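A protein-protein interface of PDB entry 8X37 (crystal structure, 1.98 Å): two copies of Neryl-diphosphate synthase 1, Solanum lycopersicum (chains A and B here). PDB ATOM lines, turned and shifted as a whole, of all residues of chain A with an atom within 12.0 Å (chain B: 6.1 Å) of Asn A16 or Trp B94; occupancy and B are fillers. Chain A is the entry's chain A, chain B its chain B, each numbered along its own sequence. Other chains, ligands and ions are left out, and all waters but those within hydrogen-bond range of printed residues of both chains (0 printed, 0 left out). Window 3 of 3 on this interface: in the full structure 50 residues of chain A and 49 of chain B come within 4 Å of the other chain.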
ATOM      1  N   SER A  12     -36.972 -39.613   7.017  1.00  0.00           N
ATOM      2  CA  SER A  12     -36.826 -40.009   5.588  1.00  0.00           C
ATOM      3  C   SER A  12     -36.035 -38.971   4.785  1.00  0.00           C
ATOM      4  O   SER A  12     -35.530 -39.288   3.715  1.00  0.00           O
ATOM      5  CB  SER A  12     -38.179 -40.285   4.949  1.00  0.00           C
ATOM      6  OG  SER A  12     -38.992 -39.121   4.918  1.00  0.00           O
ATOM      7  N   CYS A  13     -35.916 -37.744   5.307  1.00  0.00           N
ATOM      8  CA  CYS A  13     -35.379 -36.613   4.569  1.00  0.00           C
ATOM      9  C   CYS A  13     -34.163 -36.070   5.317  1.00  0.00           C
ATOM     10  O   CYS A  13     -34.183 -36.065   6.543  1.00  0.00           O
ATOM     11  CB  CYS A  13     -36.467 -35.550   4.502  1.00  0.00           C
ATOM     12  SG  CYS A  13     -36.522 -34.653   2.936  1.00  0.00           S
ATOM     13  N   SER A  14     -33.107 -35.645   4.601  1.00  0.00           N
ATOM     14  CA  SER A  14     -32.008 -34.897   5.204  1.00  0.00           C
ATOM     15  C   SER A  14     -30.952 -34.559   4.145  1.00  0.00           C
ATOM     16  O   SER A  14     -30.416 -35.476   3.529  1.00  0.00           O
ATOM     17  CB  SER A  14     -31.377 -35.655   6.365  1.00  0.00           C
ATOM     18  OG  SER A  14     -30.729 -34.749   7.243  1.00  0.00           O
ATOM     19  N   LEU A  15     -30.612 -33.267   3.982  1.00  0.00           N
ATOM     20  CA  LEU A  15     -29.764 -32.819   2.879  1.00  0.00           C
ATOM     21  C   LEU A  15     -28.635 -31.871   3.294  1.00  0.00           C
ATOM     22  O   LEU A  15     -27.689 -31.718   2.523  1.00  0.00           O
ATOM     23  CB  LEU A  15     -30.603 -32.166   1.778  1.00  0.00           C
ATOM     24  CG  LEU A  15     -31.567 -33.082   1.017  1.00  0.00           C
ATOM     25  CD1 LEU A  15     -32.228 -32.322  -0.144  1.00  0.00           C
ATOM     26  CD2 LEU A  15     -30.874 -34.340   0.503  1.00  0.00           C
ATOM     27  N   ASN A  16     -28.717 -31.205   4.454  1.00  0.00           N
ATOM     28  CA  ASN A  16     -27.714 -30.201   4.790  1.00  0.00           C
ATOM     29  C   ASN A  16     -26.516 -30.856   5.489  1.00  0.00           C
ATOM     30  O   ASN A  16     -25.370 -30.486   5.236  1.00  0.00           O
ATOM     31  CB  ASN A  16     -28.312 -29.026   5.557  1.00  0.00           C
ATOM     32  CG  ASN A  16     -29.015 -29.444   6.825  1.00  0.00           C
ATOM     33  OD1 ASN A  16     -29.153 -30.642   7.093  1.00  0.00           O
ATOM     34  ND2 ASN A  16     -29.475 -28.478   7.607  1.00  0.00           N
ATOM     35  N   LEU A  17     -26.774 -31.855   6.336  1.00  0.00           N
ATOM     36  CA  LEU A  17     -25.744 -32.451   7.174  1.00  0.00           C
ATOM     37  C   LEU A  17     -25.073 -33.621   6.433  1.00  0.00           C
ATOM     38  O   LEU A  17     -24.222 -33.321   5.569  1.00  0.00           O
ATOM     39  CB  LEU A  17     -26.377 -32.896   8.492  1.00  0.00           C
ATOM     40  CG  LEU A  17     -27.059 -31.797   9.321  1.00  0.00           C
ATOM     41  CD1 LEU A  17     -27.868 -32.365  10.479  1.00  0.00           C
ATOM     42  CD2 LEU A  17     -26.053 -30.775   9.830  1.00  0.00           C
ATOM     43  N   LYS A  21     -18.416 -36.340   0.385  1.00  0.00           N
ATOM     44  CA  LYS A  21     -17.692 -36.243  -0.912  1.00  0.00           C
ATOM     45  C   LYS A  21     -18.573 -36.779  -2.035  1.00  0.00           C
ATOM     46  O   LYS A  21     -19.317 -37.734  -1.836  1.00  0.00           O
ATOM     47  CB  LYS A  21     -16.381 -37.035  -0.863  1.00  0.00           C
ATOM     48  CG  LYS A  21     -15.390 -36.494   0.146  1.00  0.00           C
ATOM     49  CD  LYS A  21     -14.122 -37.322   0.298  1.00  0.00           C
ATOM     50  CE  LYS A  21     -13.259 -36.795   1.405  1.00  0.00           C
ATOM     51  NZ  LYS A  21     -12.123 -37.673   1.690  1.00  0.00           N
ATOM     52  N   LYS A 189     -26.178 -41.661  -2.385  1.00  0.00           N
ATOM     53  CA  LYS A 189     -25.432 -41.351  -3.602  1.00  0.00           C
ATOM     54  C   LYS A 189     -24.341 -42.384  -3.890  1.00  0.00           C
ATOM     55  O   LYS A 189     -24.204 -42.827  -5.028  1.00  0.00           O
ATOM     56  CB  LYS A 189     -24.704 -40.004  -3.534  1.00  0.00           C
ATOM     57  CG  LYS A 189     -25.474 -38.784  -3.999  1.00  0.00           C
ATOM     58  CD  LYS A 189     -24.735 -37.478  -3.741  1.00  0.00           C
ATOM     59  CE  LYS A 189     -24.422 -37.228  -2.287  1.00  0.00           C
ATOM     60  NZ  LYS A 189     -23.809 -35.918  -2.040  1.00  0.00           N
ATOM     61  N   TYR A 225     -22.470 -32.209 -12.592  1.00  0.00           N
ATOM     62  CA  TYR A 225     -21.600 -31.061 -12.378  1.00  0.00           C
ATOM     63  C   TYR A 225     -20.604 -30.890 -13.527  1.00  0.00           C
ATOM     64  O   TYR A 225     -19.689 -30.095 -13.406  1.00  0.00           O
ATOM     65  CB  TYR A 225     -20.787 -31.140 -11.081  1.00  0.00           C
ATOM     66  CG  TYR A 225     -21.597 -31.261  -9.806  1.00  0.00           C
ATOM     67  CD1 TYR A 225     -22.307 -30.184  -9.279  1.00  0.00           C
ATOM     68  CD2 TYR A 225     -21.632 -32.466  -9.123  1.00  0.00           C
ATOM     69  CE1 TYR A 225     -23.068 -30.319  -8.130  1.00  0.00           C
ATOM     70  CE2 TYR A 225     -22.398 -32.618  -7.978  1.00  0.00           C
ATOM     71  CZ  TYR A 225     -23.112 -31.544  -7.477  1.00  0.00           C
ATOM     72  OH  TYR A 225     -23.843 -31.733  -6.334  1.00  0.00           O
ATOM     73  N   PHE B  89     -33.033 -22.833  -4.639  1.00  0.00           N
ATOM     74  CA  PHE B  89     -32.035 -23.207  -3.646  1.00  0.00           C
ATOM     75  C   PHE B  89     -31.661 -24.677  -3.828  1.00  0.00           C
ATOM     76  O   PHE B  89     -32.517 -25.566  -3.794  1.00  0.00           O
ATOM     77  CB  PHE B  89     -32.582 -22.902  -2.250  1.00  0.00           C
ATOM     78  CG  PHE B  89     -31.572 -22.983  -1.111  1.00  0.00           C
ATOM     79  CD1 PHE B  89     -31.379 -24.159  -0.399  1.00  0.00           C
ATOM     80  CD2 PHE B  89     -30.864 -21.851  -0.711  1.00  0.00           C
ATOM     81  CE1 PHE B  89     -30.481 -24.203   0.661  1.00  0.00           C
ATOM     82  CE2 PHE B  89     -29.983 -21.895   0.358  1.00  0.00           C
ATOM     83  CZ  PHE B  89     -29.777 -23.074   1.029  1.00  0.00           C
ATOM     84  N   SER B  90     -30.357 -24.928  -4.008  1.00  0.00           N
ATOM     85  CA  SER B  90     -29.876 -26.259  -4.319  1.00  0.00           C
ATOM     86  C   SER B  90     -29.323 -26.916  -3.064  1.00  0.00           C
ATOM     87  O   SER B  90     -28.968 -26.229  -2.109  1.00  0.00           O
ATOM     88  CB  SER B  90     -28.837 -26.215  -5.383  1.00  0.00           C
ATOM     89  OG  SER B  90     -27.591 -25.849  -4.820  1.00  0.00           O
ATOM     90  N   THR B  91     -29.176 -28.246  -3.116  1.00  0.00           N
ATOM     91  CA  THR B  91     -28.611 -28.996  -2.002  1.00  0.00           C
ATOM     92  C   THR B  91     -27.196 -28.505  -1.695  1.00  0.00           C
ATOM     93  O   THR B  91     -26.715 -28.704  -0.583  1.00  0.00           O
ATOM     94  CB  THR B  91     -28.614 -30.505  -2.277  1.00  0.00           C
ATOM     95  OG1 THR B  91     -29.946 -30.962  -2.507  1.00  0.00           O
ATOM     96  CG2 THR B  91     -28.050 -31.308  -1.117  1.00  0.00           C
ATOM     97  N   GLU B  92     -26.531 -27.874  -2.671  1.00  0.00           N
ATOM     98  CA  GLU B  92     -25.157 -27.446  -2.489  1.00  0.00           C
ATOM     99  C   GLU B  92     -25.104 -26.036  -1.898  1.00  0.00           C
ATOM    100  O   GLU B  92     -24.047 -25.593  -1.445  1.00  0.00           O
ATOM    101  CB  GLU B  92     -24.391 -27.502  -3.810  1.00  0.00           C
ATOM    102  CG  GLU B  92     -24.088 -28.923  -4.281  1.00  0.00           C
ATOM    103  CD  GLU B  92     -25.296 -29.764  -4.691  1.00  0.00           C
ATOM    104  OE1 GLU B  92     -26.008 -29.416  -5.654  1.00  0.00           O
ATOM    105  OE2 GLU B  92     -25.514 -30.808  -4.048  1.00  0.00           O
ATOM    106  N   ASN B  93     -26.238 -25.326  -1.899  1.00  0.00           N
ATOM    107  CA  ASN B  93     -26.273 -23.952  -1.421  1.00  0.00           C
ATOM    108  C   ASN B  93     -26.085 -23.898   0.098  1.00  0.00           C
ATOM    109  O   ASN B  93     -25.724 -22.847   0.629  1.00  0.00           O
ATOM    110  CB  ASN B  93     -27.541 -23.243  -1.894  1.00  0.00           C
ATOM    111  CG  ASN B  93     -27.522 -22.905  -3.372  1.00  0.00           C
ATOM    112  OD1 ASN B  93     -28.580 -22.818  -4.006  1.00  0.00           O
ATOM    113  ND2 ASN B  93     -26.345 -22.713  -3.955  1.00  0.00           N
ATOM    114  N   TRP B  94     -26.282 -25.031   0.799  1.00  0.00           N
ATOM    115  CA  TRP B  94     -26.082 -25.069   2.242  1.00  0.00           C
ATOM    116  C   TRP B  94     -24.639 -24.730   2.605  1.00  0.00           C
ATOM    117  O   TRP B  94     -24.383 -24.354   3.744  1.00  0.00           O
ATOM    118  CB  TRP B  94     -26.442 -26.439   2.835  1.00  0.00           C
ATOM    119  CG  TRP B  94     -27.911 -26.767   2.838  1.00  0.00           C
ATOM    120  CD1 TRP B  94     -28.537 -27.669   2.031  1.00  0.00           C
ATOM    121  CD2 TRP B  94     -28.934 -26.211   3.693  1.00  0.00           C
ATOM    122  NE1 TRP B  94     -29.873 -27.722   2.327  1.00  0.00           N
ATOM    123  CE2 TRP B  94     -30.150 -26.841   3.336  1.00  0.00           C
ATOM    124  CE3 TRP B  94     -28.947 -25.260   4.721  1.00  0.00           C
ATOM    125  CZ2 TRP B  94     -31.359 -26.549   3.971  1.00  0.00           C
ATOM    126  CZ3 TRP B  94     -30.143 -24.965   5.345  1.00  0.00           C
ATOM    127  CH2 TRP B  94     -31.332 -25.606   4.979  1.00  0.00           C
ATOM    128  N   LYS B  95     -23.702 -24.889   1.657  1.00  0.00           N
ATOM    129  CA  LYS B  95     -22.288 -24.720   1.967  1.00  0.00           C
ATOM    130  C   LYS B  95     -21.867 -23.246   1.920  1.00  0.00           C
ATOM    131  O   LYS B  95     -20.738 -22.913   2.268  1.00  0.00           O
ATOM    132  CB  LYS B  95     -21.362 -25.607   1.122  1.00  0.00           C
ATOM    133  CG  LYS B  95     -21.543 -27.113   1.259  1.00  0.00           C
ATOM    134  CD  LYS B  95     -22.196 -27.622   2.545  1.00  0.00           C
ATOM    135  CE  LYS B  95     -21.467 -27.322   3.825  1.00  0.00           C
ATOM    136  NZ  LYS B  95     -22.391 -27.181   4.956  1.00  0.00           N
ATOM    137  N   ARG B  96     -22.768 -22.341   1.535  1.00  0.00           N
ATOM    138  CA  ARG B  96     -22.496 -20.916   1.643  1.00  0.00           C
ATOM    139  C   ARG B  96     -22.512 -20.499   3.122  1.00  0.00           C
ATOM    140  O   ARG B  96     -22.818 -21.297   4.009  1.00  0.00           O
ATOM    141  CB  ARG B  96     -23.463 -20.209   0.680  1.00  0.00           C
ATOM    142  CG  ARG B  96     -23.068 -20.515  -0.761  1.00  0.00           C
ATOM    143  CD  ARG B  96     -24.143 -20.427  -1.827  1.00  0.00           C
ATOM    144  NE  ARG B  96     -24.474 -19.081  -2.299  1.00  0.00           N
ATOM    145  CZ  ARG B  96     -24.756 -18.731  -3.554  1.00  0.00           C
ATOM    146  NH1 ARG B  96     -24.603 -19.581  -4.553  1.00  0.00           N
ATOM    147  NH2 ARG B  96     -25.183 -17.503  -3.809  1.00  0.00           N
ATOM    148  N   SER B  97     -22.136 -19.241   3.392  1.00  0.00           N
ATOM    149  CA  SER B  97     -21.990 -18.758   4.760  1.00  0.00           C
ATOM    150  C   SER B  97     -23.335 -18.799   5.485  1.00  0.00           C
ATOM    151  O   SER B  97     -24.378 -18.653   4.855  1.00  0.00           O
ATOM    152  CB  SER B  97     -21.408 -17.370   4.787  1.00  0.00           C
ATOM    153  OG  SER B  97     -22.374 -16.409   4.389  1.00  0.00           O
ATOM    154  N   VAL B 101     -27.017 -17.883   4.060  1.00  0.00           N
ATOM    155  CA  VAL B 101     -28.048 -18.911   4.072  1.00  0.00           C
ATOM    156  C   VAL B 101     -29.293 -18.379   4.788  1.00  0.00           C
ATOM    157  O   VAL B 101     -30.376 -18.364   4.200  1.00  0.00           O
ATOM    158  CB  VAL B 101     -27.535 -20.228   4.698  1.00  0.00           C
ATOM    159  CG1 VAL B 101     -28.639 -21.253   4.948  1.00  0.00           C
ATOM    160  CG2 VAL B 101     -26.433 -20.847   3.853  1.00  0.00           C
ATOM    161  N   LEU B 105     -33.178 -17.992   3.342  1.00  0.00           N
ATOM    162  CA  LEU B 105     -34.247 -18.829   3.877  1.00  0.00           C
ATOM    163  C   LEU B 105     -35.306 -17.964   4.552  1.00  0.00           C
ATOM    164  O   LEU B 105     -36.483 -18.321   4.558  1.00  0.00           O
ATOM    165  CB  LEU B 105     -33.739 -19.901   4.846  1.00  0.00           C
ATOM    166  CG  LEU B 105     -32.915 -21.050   4.250  1.00  0.00           C
ATOM    167  CD1 LEU B 105     -32.838 -22.186   5.265  1.00  0.00           C
ATOM    168  CD2 LEU B 105     -33.414 -21.589   2.909  1.00  0.00           C
ATOM    169  N   ASP B 130     -36.029 -30.016   6.207  1.00  0.00           N
ATOM    170  CA  ASP B 130     -34.773 -29.388   6.606  1.00  0.00           C
ATOM    171  C   ASP B 130     -34.944 -27.887   6.866  1.00  0.00           C
ATOM    172  O   ASP B 130     -34.047 -27.248   7.422  1.00  0.00           O
ATOM    173  CB  ASP B 130     -33.685 -29.548   5.550  1.00  0.00           C
ATOM    174  CG  ASP B 130     -32.982 -30.898   5.473  1.00  0.00           C
ATOM    175  OD1 ASP B 130     -33.218 -31.754   6.355  1.00  0.00           O
ATOM    176  OD2 ASP B 130     -32.184 -31.073   4.528  1.00  0.00           O
ATOM    177  N   LEU B 131     -36.067 -27.309   6.417  1.00  0.00           N
ATOM    178  CA  LEU B 131     -36.244 -25.864   6.430  1.00  0.00           C
ATOM    179  C   LEU B 131     -36.855 -25.403   7.755  1.00  0.00           C
ATOM    180  O   LEU B 131     -37.623 -26.135   8.380  1.00  0.00           O
ATOM    181  CB  LEU B 131     -37.144 -25.457   5.263  1.00  0.00           C
ATOM    182  CG  LEU B 131     -36.671 -25.846   3.860  1.00  0.00           C
ATOM    183  CD1 LEU B 131     -37.741 -25.463   2.837  1.00  0.00           C
ATOM    184  CD2 LEU B 131     -35.323 -25.229   3.512  1.00  0.00           C
ATOM    185  N   PRO B 132     -36.596 -24.148   8.192  1.00  0.00           N
ATOM    186  CA  PRO B 132     -37.284 -23.587   9.358  1.00  0.00           C
ATOM    187  C   PRO B 132     -38.793 -23.802   9.289  1.00  0.00           C
ATOM    188  O   PRO B 132     -39.396 -23.660   8.226  1.00  0.00           O
ATOM    189  CB  PRO B 132     -36.919 -22.088   9.333  1.00  0.00           C
ATOM    190  CG  PRO B 132     -35.620 -22.026   8.545  1.00  0.00           C
ATOM    191  CD  PRO B 132     -35.651 -23.202   7.577  1.00  0.00           C
ATOM    192  N   ASN B 159     -34.378 -26.377  -1.704  1.00  0.00           N
ATOM    193  CA  ASN B 159     -33.656 -27.491  -1.111  1.00  0.00           C
ATOM    194  C   ASN B 159     -33.839 -28.738  -1.974  1.00  0.00           C
ATOM    195  O   ASN B 159     -34.229 -29.790  -1.489  1.00  0.00           O
ATOM    196  CB  ASN B 159     -34.058 -27.709   0.342  1.00  0.00           C
ATOM    197  CG  ASN B 159     -33.041 -28.538   1.091  1.00  0.00           C
ATOM    198  OD1 ASN B 159     -31.835 -28.388   0.892  1.00  0.00           O
ATOM    199  ND2 ASN B 159     -33.494 -29.420   1.961  1.00  0.00           N
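No position is printed for both chains.
N of Leu A15 sits at hydrogen-bond distance from OD2 of Asp B130.
The backbone NH of Asn A16 is in hydrogen-bond range of the side-chain carboxylate of Asp B130 (3.5 Å).
The side-chain carboxylate of Glu B92 sits close to the side-chain hydroxyl of Tyr A225 (3.0 Å).
Of the 9 printed residues of chain A, 4 touch a printed residue of chain B.
Printed residues of chain A that touch a printed residue of chain B: Ser A14, Leu A15, Asn A16 and Tyr A225.
Hydrophobic or aromatic side chains of chain A that line the printed part of chain B: Leu A15 and Tyr A225.
Among the printed residues, 7 pairs touch across the chains.
Among the printed residues, no Asp or Glu carboxylate lies within 4 Å of a Lys or Arg side-chain nitrogen of the other chain.
Asn A16 touches two residues of chain B.
Trp B94 touches just one residue of chain A: Asn A16.
Glu B92 touches just one residue of chain A: Tyr A225.
Asn B93 touches none of the printed residues of chain A.
No residue of chain A comes within 4 Å of Lys B95.
No residue of chain A comes within 4 Å of Val B101.
Asp B130 touches three residues of chain A.
No residue of chain A comes within 4 Å of Leu B131.
Of chain A, only Leu A15 (3.5 Å) comes within 4 Å of Asn B159.
Printed residues of chain B within 4 Å of Tyr A225: Glu B92 (2.9 Å).
Printed residues of chain B within 4 Å of Leu A15: Thr B91, Asp B130 and Asn B159.
The nearest residue of chain B that does not touch Asn A16 is Lys B95 (4.5 Å).
The nearest residue of chain A that does not touch Trp B94 is Leu A15 (4.2 Å).
The nearest printed residue of chain B that does not touch Tyr A225 is Thr B91 (6.4 Å).
Ser A14 touches Asp B130.
Thr B91 touches Leu A15.
Leu A15 touches Asn B159.
Trp B94 touches Asn A16 (CD2 to CB, 3.4 Å).
The backbone carbonyl oxygen (O) of Phe B89 is in hydrogen-bond range of the backbone NH (N) of Asn B159, 2.9 Å away.
OG of Ser B90 sits close to N of Glu B92, at 3.1 Å.
The indole nitrogen (NE1) of Trp B94 lies within hydrogen-bond range of the side-chain amide oxygen (OD1) of Asn B159, at 2.5 Å.
The side-chain carboxylate (OD2) of Asp B130 is in hydrogen-bond range of the side-chain amide nitrogen (ND2) of Asn B159, at 3.3 Å.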
